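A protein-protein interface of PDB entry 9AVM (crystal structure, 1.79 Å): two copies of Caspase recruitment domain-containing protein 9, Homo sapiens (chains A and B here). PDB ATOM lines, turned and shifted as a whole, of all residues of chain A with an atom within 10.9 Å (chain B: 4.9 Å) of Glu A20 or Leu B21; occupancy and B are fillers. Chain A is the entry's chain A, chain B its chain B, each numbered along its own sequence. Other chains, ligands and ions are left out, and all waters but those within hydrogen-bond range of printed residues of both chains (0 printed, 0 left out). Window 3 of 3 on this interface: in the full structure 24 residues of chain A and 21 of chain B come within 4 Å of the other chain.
Printed residues of chain B that touch a printed residue of chain A: Glu B20, Leu B21, Cys B24 and Lys B25. Of the 17 printed residues of chain A, 4 touch a printed residue of chain B. Hydrophobic or aromatic side chains of chain A that line the printed part of chain B: Leu A21. Among the printed residues, 9 pairs touch across the chains.
Lys A22 touches none of the printed residues of chain B. Of the printed residues of chain B, Cys A24 touches Leu B21, Cys B24 and Lys B25. Printed residues of chain B within 4 Å of Lys A25: Glu B20 and Cys B24. No residue of chain A comes within 4 Å of Gly B17. No residue of chain A comes within 4 Å of Ser B18. Cys B24 touches just these residues of chain A: Cys A24 (2.9 Å) and Lys A25 (3.8 Å). Lys B25 touches two residues of chain A. The nearest residue of chain A that does not touch Leu B21 is Gly A17 (4.2 Å). The nearest printed residue of chain B that does not touch Cys A24 is Glu B20 (6.2 Å).
Among the printed residues, merely in contact across the chains: Leu A21 with Glu B20, Glu A20 with Leu B21, Leu A21 with Leu B21 and Cys A24 with Leu B21.
Glu A20 touches Lys B25, and with the chains exchanged Lys A25 touches Glu B20. Leu A21 touches its own counterpart, Leu B21. Cys A24 touches Leu B21, but with the chains exchanged Leu A21 does not touch Cys B24 (4.5 Å). Cys B24 touches its own counterpart, Cys A24. Of the 9 pairs that touch across the chains among the printed residues, 8 have their exchanged pair printed and touching as well.
The side-chain sulfur of Cys A24 is in hydrogen-bond range of the backbone NH of Lys B25. The side-chain carboxylate (OE2) of Glu A20 lies within salt-bridge range of the side-chain amino group (NZ) of Lys B25 (3.3 Å). N of Lys A25 lies within hydrogen-bond range of SG of Cys B24, 3.8 Å away. The side-chain sulfur (SG) of Cys B24 sits at hydrogen-bond distance from the backbone carbonyl oxygen (O) of Cys A24 (3.4 Å). The side-chain carboxylate of Glu B20 is in salt-bridge range of the side-chain amino group of Lys A25 (3.5 Å).
The side-chain carboxylate (OE2) of Glu A20 is in salt-bridge range of the guanidinium group (NH2) of Arg A23.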
ATOM      1  N   GLU A  12     -24.362 -21.234 -19.520  1.00  0.00           N
ATOM      2  CA  GLU A  12     -24.675 -21.396 -20.941  1.00  0.00           C
ATOM      3  C   GLU A  12     -23.531 -20.938 -21.849  1.00  0.00           C
ATOM      4  O   GLU A  12     -23.221 -21.636 -22.811  1.00  0.00           O
ATOM      5  CB  GLU A  12     -26.001 -20.710 -21.311  1.00  0.00           C
ATOM      6  CG  GLU A  12     -26.125 -19.282 -20.802  1.00  0.00           C
ATOM      7  CD  GLU A  12     -27.475 -18.641 -21.052  1.00  0.00           C
ATOM      8  OE1 GLU A  12     -28.475 -19.118 -20.468  1.00  0.00           O
ATOM      9  OE2 GLU A  12     -27.533 -17.662 -21.831  1.00  0.00           O
ATOM     10  N   GLU A  13     -22.898 -19.790 -21.541  1.00  0.00           N
ATOM     11  CA  GLU A  13     -21.765 -19.283 -22.320  1.00  0.00           C
ATOM     12  C   GLU A  13     -20.554 -20.219 -22.200  1.00  0.00           C
ATOM     13  O   GLU A  13     -19.802 -20.383 -23.159  1.00  0.00           O
ATOM     14  CB  GLU A  13     -21.381 -17.859 -21.881  1.00  0.00           C
ATOM     15  CG  GLU A  13     -22.307 -16.775 -22.411  1.00  0.00           C
ATOM     16  CD  GLU A  13     -21.865 -15.350 -22.128  1.00  0.00           C
ATOM     17  OE1 GLU A  13     -22.515 -14.412 -22.643  1.00  0.00           O
ATOM     18  OE2 GLU A  13     -20.868 -15.168 -21.391  1.00  0.00           O
ATOM     19  N   CYS A  14     -20.385 -20.853 -21.038  1.00  0.00           N
ATOM     20  CA  CYS A  14     -19.288 -21.768 -20.810  1.00  0.00           C
ATOM     21  C   CYS A  14     -19.519 -23.129 -21.480  1.00  0.00           C
ATOM     22  O   CYS A  14     -18.563 -23.744 -21.932  1.00  0.00           O
ATOM     23  CB  CYS A  14     -19.009 -21.894 -19.321  1.00  0.00           C
ATOM     24  SG  CYS A  14     -18.647 -20.310 -18.507  1.00  0.00           S
ATOM     25  N   GLU A  15     -20.773 -23.570 -21.594  1.00  0.00           N
ATOM     26  CA  GLU A  15     -21.096 -24.805 -22.318  1.00  0.00           C
ATOM     27  C   GLU A  15     -20.858 -24.584 -23.820  1.00  0.00           C
ATOM     28  O   GLU A  15     -20.367 -25.485 -24.500  1.00  0.00           O
ATOM     29  CB  GLU A  15     -22.569 -25.205 -22.092  1.00  0.00           C
ATOM     30  CG  GLU A  15     -22.814 -25.847 -20.745  1.00  0.00           C
ATOM     31  CD  GLU A  15     -24.258 -25.882 -20.289  1.00  0.00           C
ATOM     32  OE1 GLU A  15     -25.126 -25.299 -20.982  1.00  0.00           O
ATOM     33  OE2 GLU A  15     -24.516 -26.486 -19.222  1.00  0.00           O
ATOM     34  N   ALA A  16     -21.223 -23.382 -24.326  1.00  0.00           N
ATOM     35  CA  ALA A  16     -21.060 -22.995 -25.724  1.00  0.00           C
ATOM     36  C   ALA A  16     -19.569 -22.893 -26.065  1.00  0.00           C
ATOM     37  O   ALA A  16     -19.151 -23.372 -27.121  1.00  0.00           O
ATOM     38  CB  ALA A  16     -21.758 -21.665 -25.990  1.00  0.00           C
ATOM     39  N   GLY A  17     -18.784 -22.321 -25.148  1.00  0.00           N
ATOM     40  CA  GLY A  17     -17.339 -22.211 -25.296  1.00  0.00           C
ATOM     41  C   GLY A  17     -16.646 -23.560 -25.358  1.00  0.00           C
ATOM     42  O   GLY A  17     -15.738 -23.743 -26.172  1.00  0.00           O
ATOM     43  N   SER A  18     -17.072 -24.545 -24.535  1.00  0.00           N
ATOM     44  CA  SER A  18     -16.446 -25.876 -24.563  1.00  0.00           C
ATOM     45  C   SER A  18     -16.794 -26.643 -25.866  1.00  0.00           C
ATOM     46  O   SER A  18     -15.977 -27.413 -26.374  1.00  0.00           O
ATOM     47  CB  SER A  18     -16.780 -26.665 -23.295  1.00  0.00           C
ATOM     48  OG  SER A  18     -17.891 -27.538 -23.424  1.00  0.00           O
ATOM     49  N   ARG A  19     -17.981 -26.371 -26.437  1.00  0.00           N
ATOM     50  CA  ARG A  19     -18.351 -26.964 -27.718  1.00  0.00           C
ATOM     51  C   ARG A  19     -17.537 -26.306 -28.849  1.00  0.00           C
ATOM     52  O   ARG A  19     -17.038 -27.000 -29.732  1.00  0.00           O
ATOM     53  CB  ARG A  19     -19.860 -26.834 -27.968  1.00  0.00           C
ATOM     54  CG  ARG A  19     -20.670 -27.785 -27.088  1.00  0.00           C
ATOM     55  CD  ARG A  19     -22.137 -27.820 -27.481  1.00  0.00           C
ATOM     56  NE  ARG A  19     -22.944 -26.873 -26.712  1.00  0.00           N
ATOM     57  CZ  ARG A  19     -23.297 -25.665 -27.135  1.00  0.00           C
ATOM     58  NH1 ARG A  19     -22.938 -25.245 -28.343  1.00  0.00           N
ATOM     59  NH2 ARG A  19     -24.028 -24.874 -26.363  1.00  0.00           N
ATOM     60  N   GLU A  20     -17.340 -24.992 -28.777  1.00  0.00           N
ATOM     61  CA  GLU A  20     -16.533 -24.269 -29.751  1.00  0.00           C
ATOM     62  C   GLU A  20     -15.055 -24.689 -29.662  1.00  0.00           C
ATOM     63  O   GLU A  20     -14.388 -24.770 -30.699  1.00  0.00           O
ATOM     64  CB  GLU A  20     -16.666 -22.756 -29.575  1.00  0.00           C
ATOM     65  CG  GLU A  20     -16.007 -21.984 -30.700  1.00  0.00           C
ATOM     66  CD  GLU A  20     -16.392 -20.527 -30.846  1.00  0.00           C
ATOM     67  OE1 GLU A  20     -16.827 -19.924 -29.835  1.00  0.00           O
ATOM     68  OE2 GLU A  20     -16.262 -19.991 -31.972  1.00  0.00           O
ATOM     69  N   LEU A  21     -14.560 -24.990 -28.457  1.00  0.00           N
ATOM     70  CA  LEU A  21     -13.173 -25.441 -28.280  1.00  0.00           C
ATOM     71  C   LEU A  21     -12.973 -26.812 -28.950  1.00  0.00           C
ATOM     72  O   LEU A  21     -11.977 -27.021 -29.662  1.00  0.00           O
ATOM     73  CB  LEU A  21     -12.803 -25.511 -26.805  1.00  0.00           C
ATOM     74  CG  LEU A  21     -11.392 -26.044 -26.490  1.00  0.00           C
ATOM     75  CD1 LEU A  21     -10.284 -25.162 -27.134  1.00  0.00           C
ATOM     76  CD2 LEU A  21     -11.187 -26.161 -25.008  1.00  0.00           C
ATOM     77  N   LYS A  22     -13.951 -27.721 -28.781  1.00  0.00           N
ATOM     78  CA  LYS A  22     -13.921 -29.050 -29.423  1.00  0.00           C
ATOM     79  C   LYS A  22     -13.836 -28.896 -30.968  1.00  0.00           C
ATOM     80  O   LYS A  22     -13.032 -29.566 -31.618  1.00  0.00           O
ATOM     81  CB  LYS A  22     -15.182 -29.853 -29.015  1.00  0.00           C
ATOM     82  CG  LYS A  22     -15.409 -31.124 -29.847  1.00  0.00           C
ATOM     83  CD  LYS A  22     -16.519 -31.995 -29.304  1.00  0.00           C
ATOM     84  CE  LYS A  22     -16.528 -33.338 -29.993  1.00  0.00           C
ATOM     85  NZ  LYS A  22     -17.078 -33.225 -31.354  1.00  0.00           N
ATOM     86  N   ARG A  23     -14.665 -28.024 -31.552  1.00  0.00           N
ATOM     87  CA  ARG A  23     -14.623 -27.774 -32.992  1.00  0.00           C
ATOM     88  C   ARG A  23     -13.279 -27.129 -33.434  1.00  0.00           C
ATOM     89  O   ARG A  23     -12.727 -27.484 -34.495  1.00  0.00           O
ATOM     90  CB  ARG A  23     -15.818 -26.920 -33.450  1.00  0.00           C
ATOM     91  CG  ARG A  23     -15.924 -26.880 -34.990  1.00  0.00           C
ATOM     92  CD  ARG A  23     -17.074 -26.035 -35.548  1.00  0.00           C
ATOM     93  NE  ARG A  23     -17.216 -24.740 -34.878  1.00  0.00           N
ATOM     94  CZ  ARG A  23     -16.455 -23.678 -35.116  1.00  0.00           C
ATOM     95  NH1 ARG A  23     -15.480 -23.739 -36.016  1.00  0.00           N
ATOM     96  NH2 ARG A  23     -16.667 -22.544 -34.460  1.00  0.00           N
ATOM     97  N   CYS A  24     -12.755 -26.190 -32.634  1.00  0.00           N
ATOM     98  CA  CYS A  24     -11.508 -25.517 -32.971  1.00  0.00           C
ATOM     99  C   CYS A  24     -10.332 -26.502 -32.994  1.00  0.00           C
ATOM    100  O   CYS A  24      -9.483 -26.434 -33.879  1.00  0.00           O
ATOM    101  CB  CYS A  24     -11.258 -24.373 -31.995  1.00  0.00           C
ATOM    102  SG  CYS A  24     -10.034 -23.175 -32.558  1.00  0.00           S
ATOM    103  N   LYS A  25     -10.303 -27.446 -32.046  1.00  0.00           N
ATOM    104  CA  LYS A  25      -9.236 -28.451 -31.995  1.00  0.00           C
ATOM    105  C   LYS A  25      -9.304 -29.411 -33.206  1.00  0.00           C
ATOM    106  O   LYS A  25      -8.267 -29.787 -33.774  1.00  0.00           O
ATOM    107  CB  LYS A  25      -9.294 -29.212 -30.675  1.00  0.00           C
ATOM    108  CG  LYS A  25      -8.813 -28.381 -29.488  1.00  0.00           C
ATOM    109  CD  LYS A  25      -8.906 -29.236 -28.243  1.00  0.00           C
ATOM    110  CE  LYS A  25      -8.324 -28.585 -27.021  1.00  0.00           C
ATOM    111  NZ  LYS A  25      -8.645 -29.381 -25.805  1.00  0.00           N
ATOM    112  N   GLU A  26     -10.536 -29.762 -33.627  1.00  0.00           N
ATOM    113  CA  GLU A  26     -10.748 -30.590 -34.825  1.00  0.00           C
ATOM    114  C   GLU A  26     -10.259 -29.860 -36.065  1.00  0.00           C
ATOM    115  O   GLU A  26      -9.591 -30.466 -36.900  1.00  0.00           O
ATOM    116  CB  GLU A  26     -12.238 -30.946 -34.985  1.00  0.00           C
ATOM    117  CG  GLU A  26     -12.710 -31.971 -33.966  1.00  0.00           C
ATOM    118  CD  GLU A  26     -14.214 -32.121 -33.850  1.00  0.00           C
ATOM    119  OE1 GLU A  26     -14.953 -31.303 -34.447  1.00  0.00           O
ATOM    120  OE2 GLU A  26     -14.655 -33.056 -33.147  1.00  0.00           O
ATOM    121  N   GLU A  27     -10.561 -28.545 -36.164  1.00  0.00           N
ATOM    122  CA  GLU A  27     -10.115 -27.708 -37.262  1.00  0.00           C
ATOM    123  C   GLU A  27      -8.610 -27.569 -37.264  1.00  0.00           C
ATOM    124  O   GLU A  27      -8.034 -27.517 -38.338  1.00  0.00           O
ATOM    125  CB  GLU A  27     -10.702 -26.309 -37.193  1.00  0.00           C
ATOM    126  CG  GLU A  27     -12.120 -26.195 -37.655  1.00  0.00           C
ATOM    127  CD  GLU A  27     -12.296 -24.725 -37.957  1.00  0.00           C
ATOM    128  OE1 GLU A  27     -12.428 -23.933 -37.001  1.00  0.00           O
ATOM    129  OE2 GLU A  27     -12.173 -24.357 -39.147  1.00  0.00           O
ATOM    130  N   ASN A  28      -7.969 -27.499 -36.097  1.00  0.00           N
ATOM    131  CA  ASN A  28      -6.516 -27.376 -36.007  1.00  0.00           C
ATOM    132  C   ASN A  28      -5.839 -28.614 -36.603  1.00  0.00           C
ATOM    133  O   ASN A  28      -4.880 -28.471 -37.367  1.00  0.00           O
ATOM    134  CB  ASN A  28      -6.066 -27.137 -34.543  1.00  0.00           C
ATOM    135  CG  ASN A  28      -4.565 -26.942 -34.418  1.00  0.00           C
ATOM    136  OD1 ASN A  28      -4.022 -25.827 -34.556  1.00  0.00           O
ATOM    137  ND2 ASN A  28      -3.861 -28.026 -34.162  1.00  0.00           N
ATOM    138  N   GLY B  17     -10.813 -22.577 -20.281  1.00  0.00           N
ATOM    139  CA  GLY B  17     -11.303 -22.982 -21.593  1.00  0.00           C
ATOM    140  C   GLY B  17     -11.438 -21.801 -22.537  1.00  0.00           C
ATOM    141  O   GLY B  17     -11.103 -21.911 -23.718  1.00  0.00           O
ATOM    142  N   SER B  18     -11.882 -20.650 -22.015  1.00  0.00           N
ATOM    143  CA  SER B  18     -12.004 -19.430 -22.815  1.00  0.00           C
ATOM    144  C   SER B  18     -10.624 -18.933 -23.302  1.00  0.00           C
ATOM    145  O   SER B  18     -10.506 -18.365 -24.400  1.00  0.00           O
ATOM    146  CB  SER B  18     -12.718 -18.340 -22.021  1.00  0.00           C
ATOM    147  OG  SER B  18     -13.048 -17.228 -22.839  1.00  0.00           O
ATOM    148  N   ARG B  19      -9.583 -19.168 -22.489  1.00  0.00           N
ATOM    149  CA  ARG B  19      -8.223 -18.800 -22.839  1.00  0.00           C
ATOM    150  C   ARG B  19      -7.652 -19.794 -23.852  1.00  0.00           C
ATOM    151  O   ARG B  19      -6.989 -19.380 -24.800  1.00  0.00           O
ATOM    152  CB  ARG B  19      -7.335 -18.713 -21.589  1.00  0.00           C
ATOM    153  CG  ARG B  19      -7.604 -17.462 -20.759  1.00  0.00           C
ATOM    154  CD  ARG B  19      -6.584 -17.276 -19.646  1.00  0.00           C
ATOM    155  NE  ARG B  19      -7.027 -17.874 -18.383  1.00  0.00           N
ATOM    156  CZ  ARG B  19      -6.635 -19.065 -17.939  1.00  0.00           C
ATOM    157  NH1 ARG B  19      -5.772 -19.794 -18.640  1.00  0.00           N
ATOM    158  NH2 ARG B  19      -7.085 -19.529 -16.782  1.00  0.00           N
ATOM    159  N   GLU B  20      -7.925 -21.098 -23.667  1.00  0.00           N
ATOM    160  CA  GLU B  20      -7.464 -22.121 -24.599  1.00  0.00           C
ATOM    161  C   GLU B  20      -8.132 -21.957 -25.986  1.00  0.00           C
ATOM    162  O   GLU B  20      -7.477 -22.171 -27.014  1.00  0.00           O
ATOM    163  CB  GLU B  20      -7.714 -23.523 -24.037  1.00  0.00           C
ATOM    164  CG  GLU B  20      -7.113 -24.619 -24.900  1.00  0.00           C
ATOM    165  CD  GLU B  20      -7.184 -26.027 -24.339  1.00  0.00           C
ATOM    166  OE1 GLU B  20      -8.027 -26.284 -23.449  1.00  0.00           O
ATOM    167  OE2 GLU B  20      -6.392 -26.879 -24.803  1.00  0.00           O
ATOM    168  N   LEU B  21      -9.406 -21.545 -26.016  1.00  0.00           N
ATOM    169  CA  LEU B  21     -10.112 -21.333 -27.285  1.00  0.00           C
ATOM    170  C   LEU B  21      -9.487 -20.155 -28.037  1.00  0.00           C
ATOM    171  O   LEU B  21      -9.262 -20.239 -29.243  1.00  0.00           O
ATOM    172  CB  LEU B  21     -11.609 -21.073 -27.032  1.00  0.00           C
ATOM    173  CG  LEU B  21     -12.448 -20.701 -28.266  1.00  0.00           C
ATOM    174  CD1 LEU B  21     -12.418 -21.824 -29.314  1.00  0.00           C
ATOM    175  CD2 LEU B  21     -13.859 -20.333 -27.862  1.00  0.00           C
ATOM    176  N   LYS B  22      -9.150 -19.077 -27.314  1.00  0.00           N
ATOM    177  CA  LYS B  22      -8.504 -17.895 -27.885  1.00  0.00           C
ATOM    178  C   LYS B  22      -7.168 -18.281 -28.538  1.00  0.00           C
ATOM    179  O   LYS B  22      -6.880 -17.853 -29.653  1.00  0.00           O
ATOM    180  CB  LYS B  22      -8.276 -16.839 -26.779  1.00  0.00           C
ATOM    181  CG  LYS B  22      -7.509 -15.607 -27.247  1.00  0.00           C
ATOM    182  CD  LYS B  22      -7.443 -14.533 -26.172  1.00  0.00           C
ATOM    183  CE  LYS B  22      -6.558 -13.379 -26.573  1.00  0.00           C
ATOM    184  NZ  LYS B  22      -7.034 -12.707 -27.807  1.00  0.00           N
ATOM    185  N   ARG B  23      -6.394 -19.137 -27.866  1.00  0.00           N
ATOM    186  CA  ARG B  23      -5.106 -19.635 -28.331  1.00  0.00           C
ATOM    187  C   ARG B  23      -5.279 -20.489 -29.591  1.00  0.00           C
ATOM    188  O   ARG B  23      -4.525 -20.349 -30.557  1.00  0.00           O
ATOM    189  CB  ARG B  23      -4.490 -20.490 -27.224  1.00  0.00           C
ATOM    190  CG  ARG B  23      -2.990 -20.646 -27.269  1.00  0.00           C
ATOM    191  CD  ARG B  23      -2.516 -21.303 -25.977  1.00  0.00           C
ATOM    192  NE  ARG B  23      -2.994 -20.583 -24.791  1.00  0.00           N
ATOM    193  CZ  ARG B  23      -3.651 -21.145 -23.779  1.00  0.00           C
ATOM    194  NH1 ARG B  23      -3.890 -22.453 -23.776  1.00  0.00           N
ATOM    195  NH2 ARG B  23      -4.051 -20.410 -22.754  1.00  0.00           N
ATOM    196  N   CYS B  24      -6.282 -21.366 -29.569  1.00  0.00           N
ATOM    197  CA  CYS B  24      -6.554 -22.266 -30.667  1.00  0.00           C
ATOM    198  C   CYS B  24      -6.971 -21.495 -31.928  1.00  0.00           C
ATOM    199  O   CYS B  24      -6.500 -21.815 -33.015  1.00  0.00           O
ATOM    200  CB  CYS B  24      -7.597 -23.301 -30.246  1.00  0.00           C
ATOM    201  SG  CYS B  24      -7.847 -24.632 -31.454  1.00  0.00           S
ATOM    202  N   LYS B  25      -7.811 -20.461 -31.782  1.00  0.00           N
ATOM    203  CA  LYS B  25      -8.248 -19.657 -32.917  1.00  0.00           C
ATOM    204  C   LYS B  25      -7.091 -18.886 -33.529  1.00  0.00           C
ATOM    205  O   LYS B  25      -7.001 -18.827 -34.750  1.00  0.00           O
ATOM    206  CB  LYS B  25      -9.371 -18.713 -32.512  1.00  0.00           C
ATOM    207  CG  LYS B  25     -10.708 -19.386 -32.276  1.00  0.00           C
ATOM    208  CD  LYS B  25     -11.700 -18.319 -31.892  1.00  0.00           C
ATOM    209  CE  LYS B  25     -13.122 -18.805 -31.772  1.00  0.00           C
ATOM    210  NZ  LYS B  25     -14.009 -17.755 -31.172  1.00  0.00           N
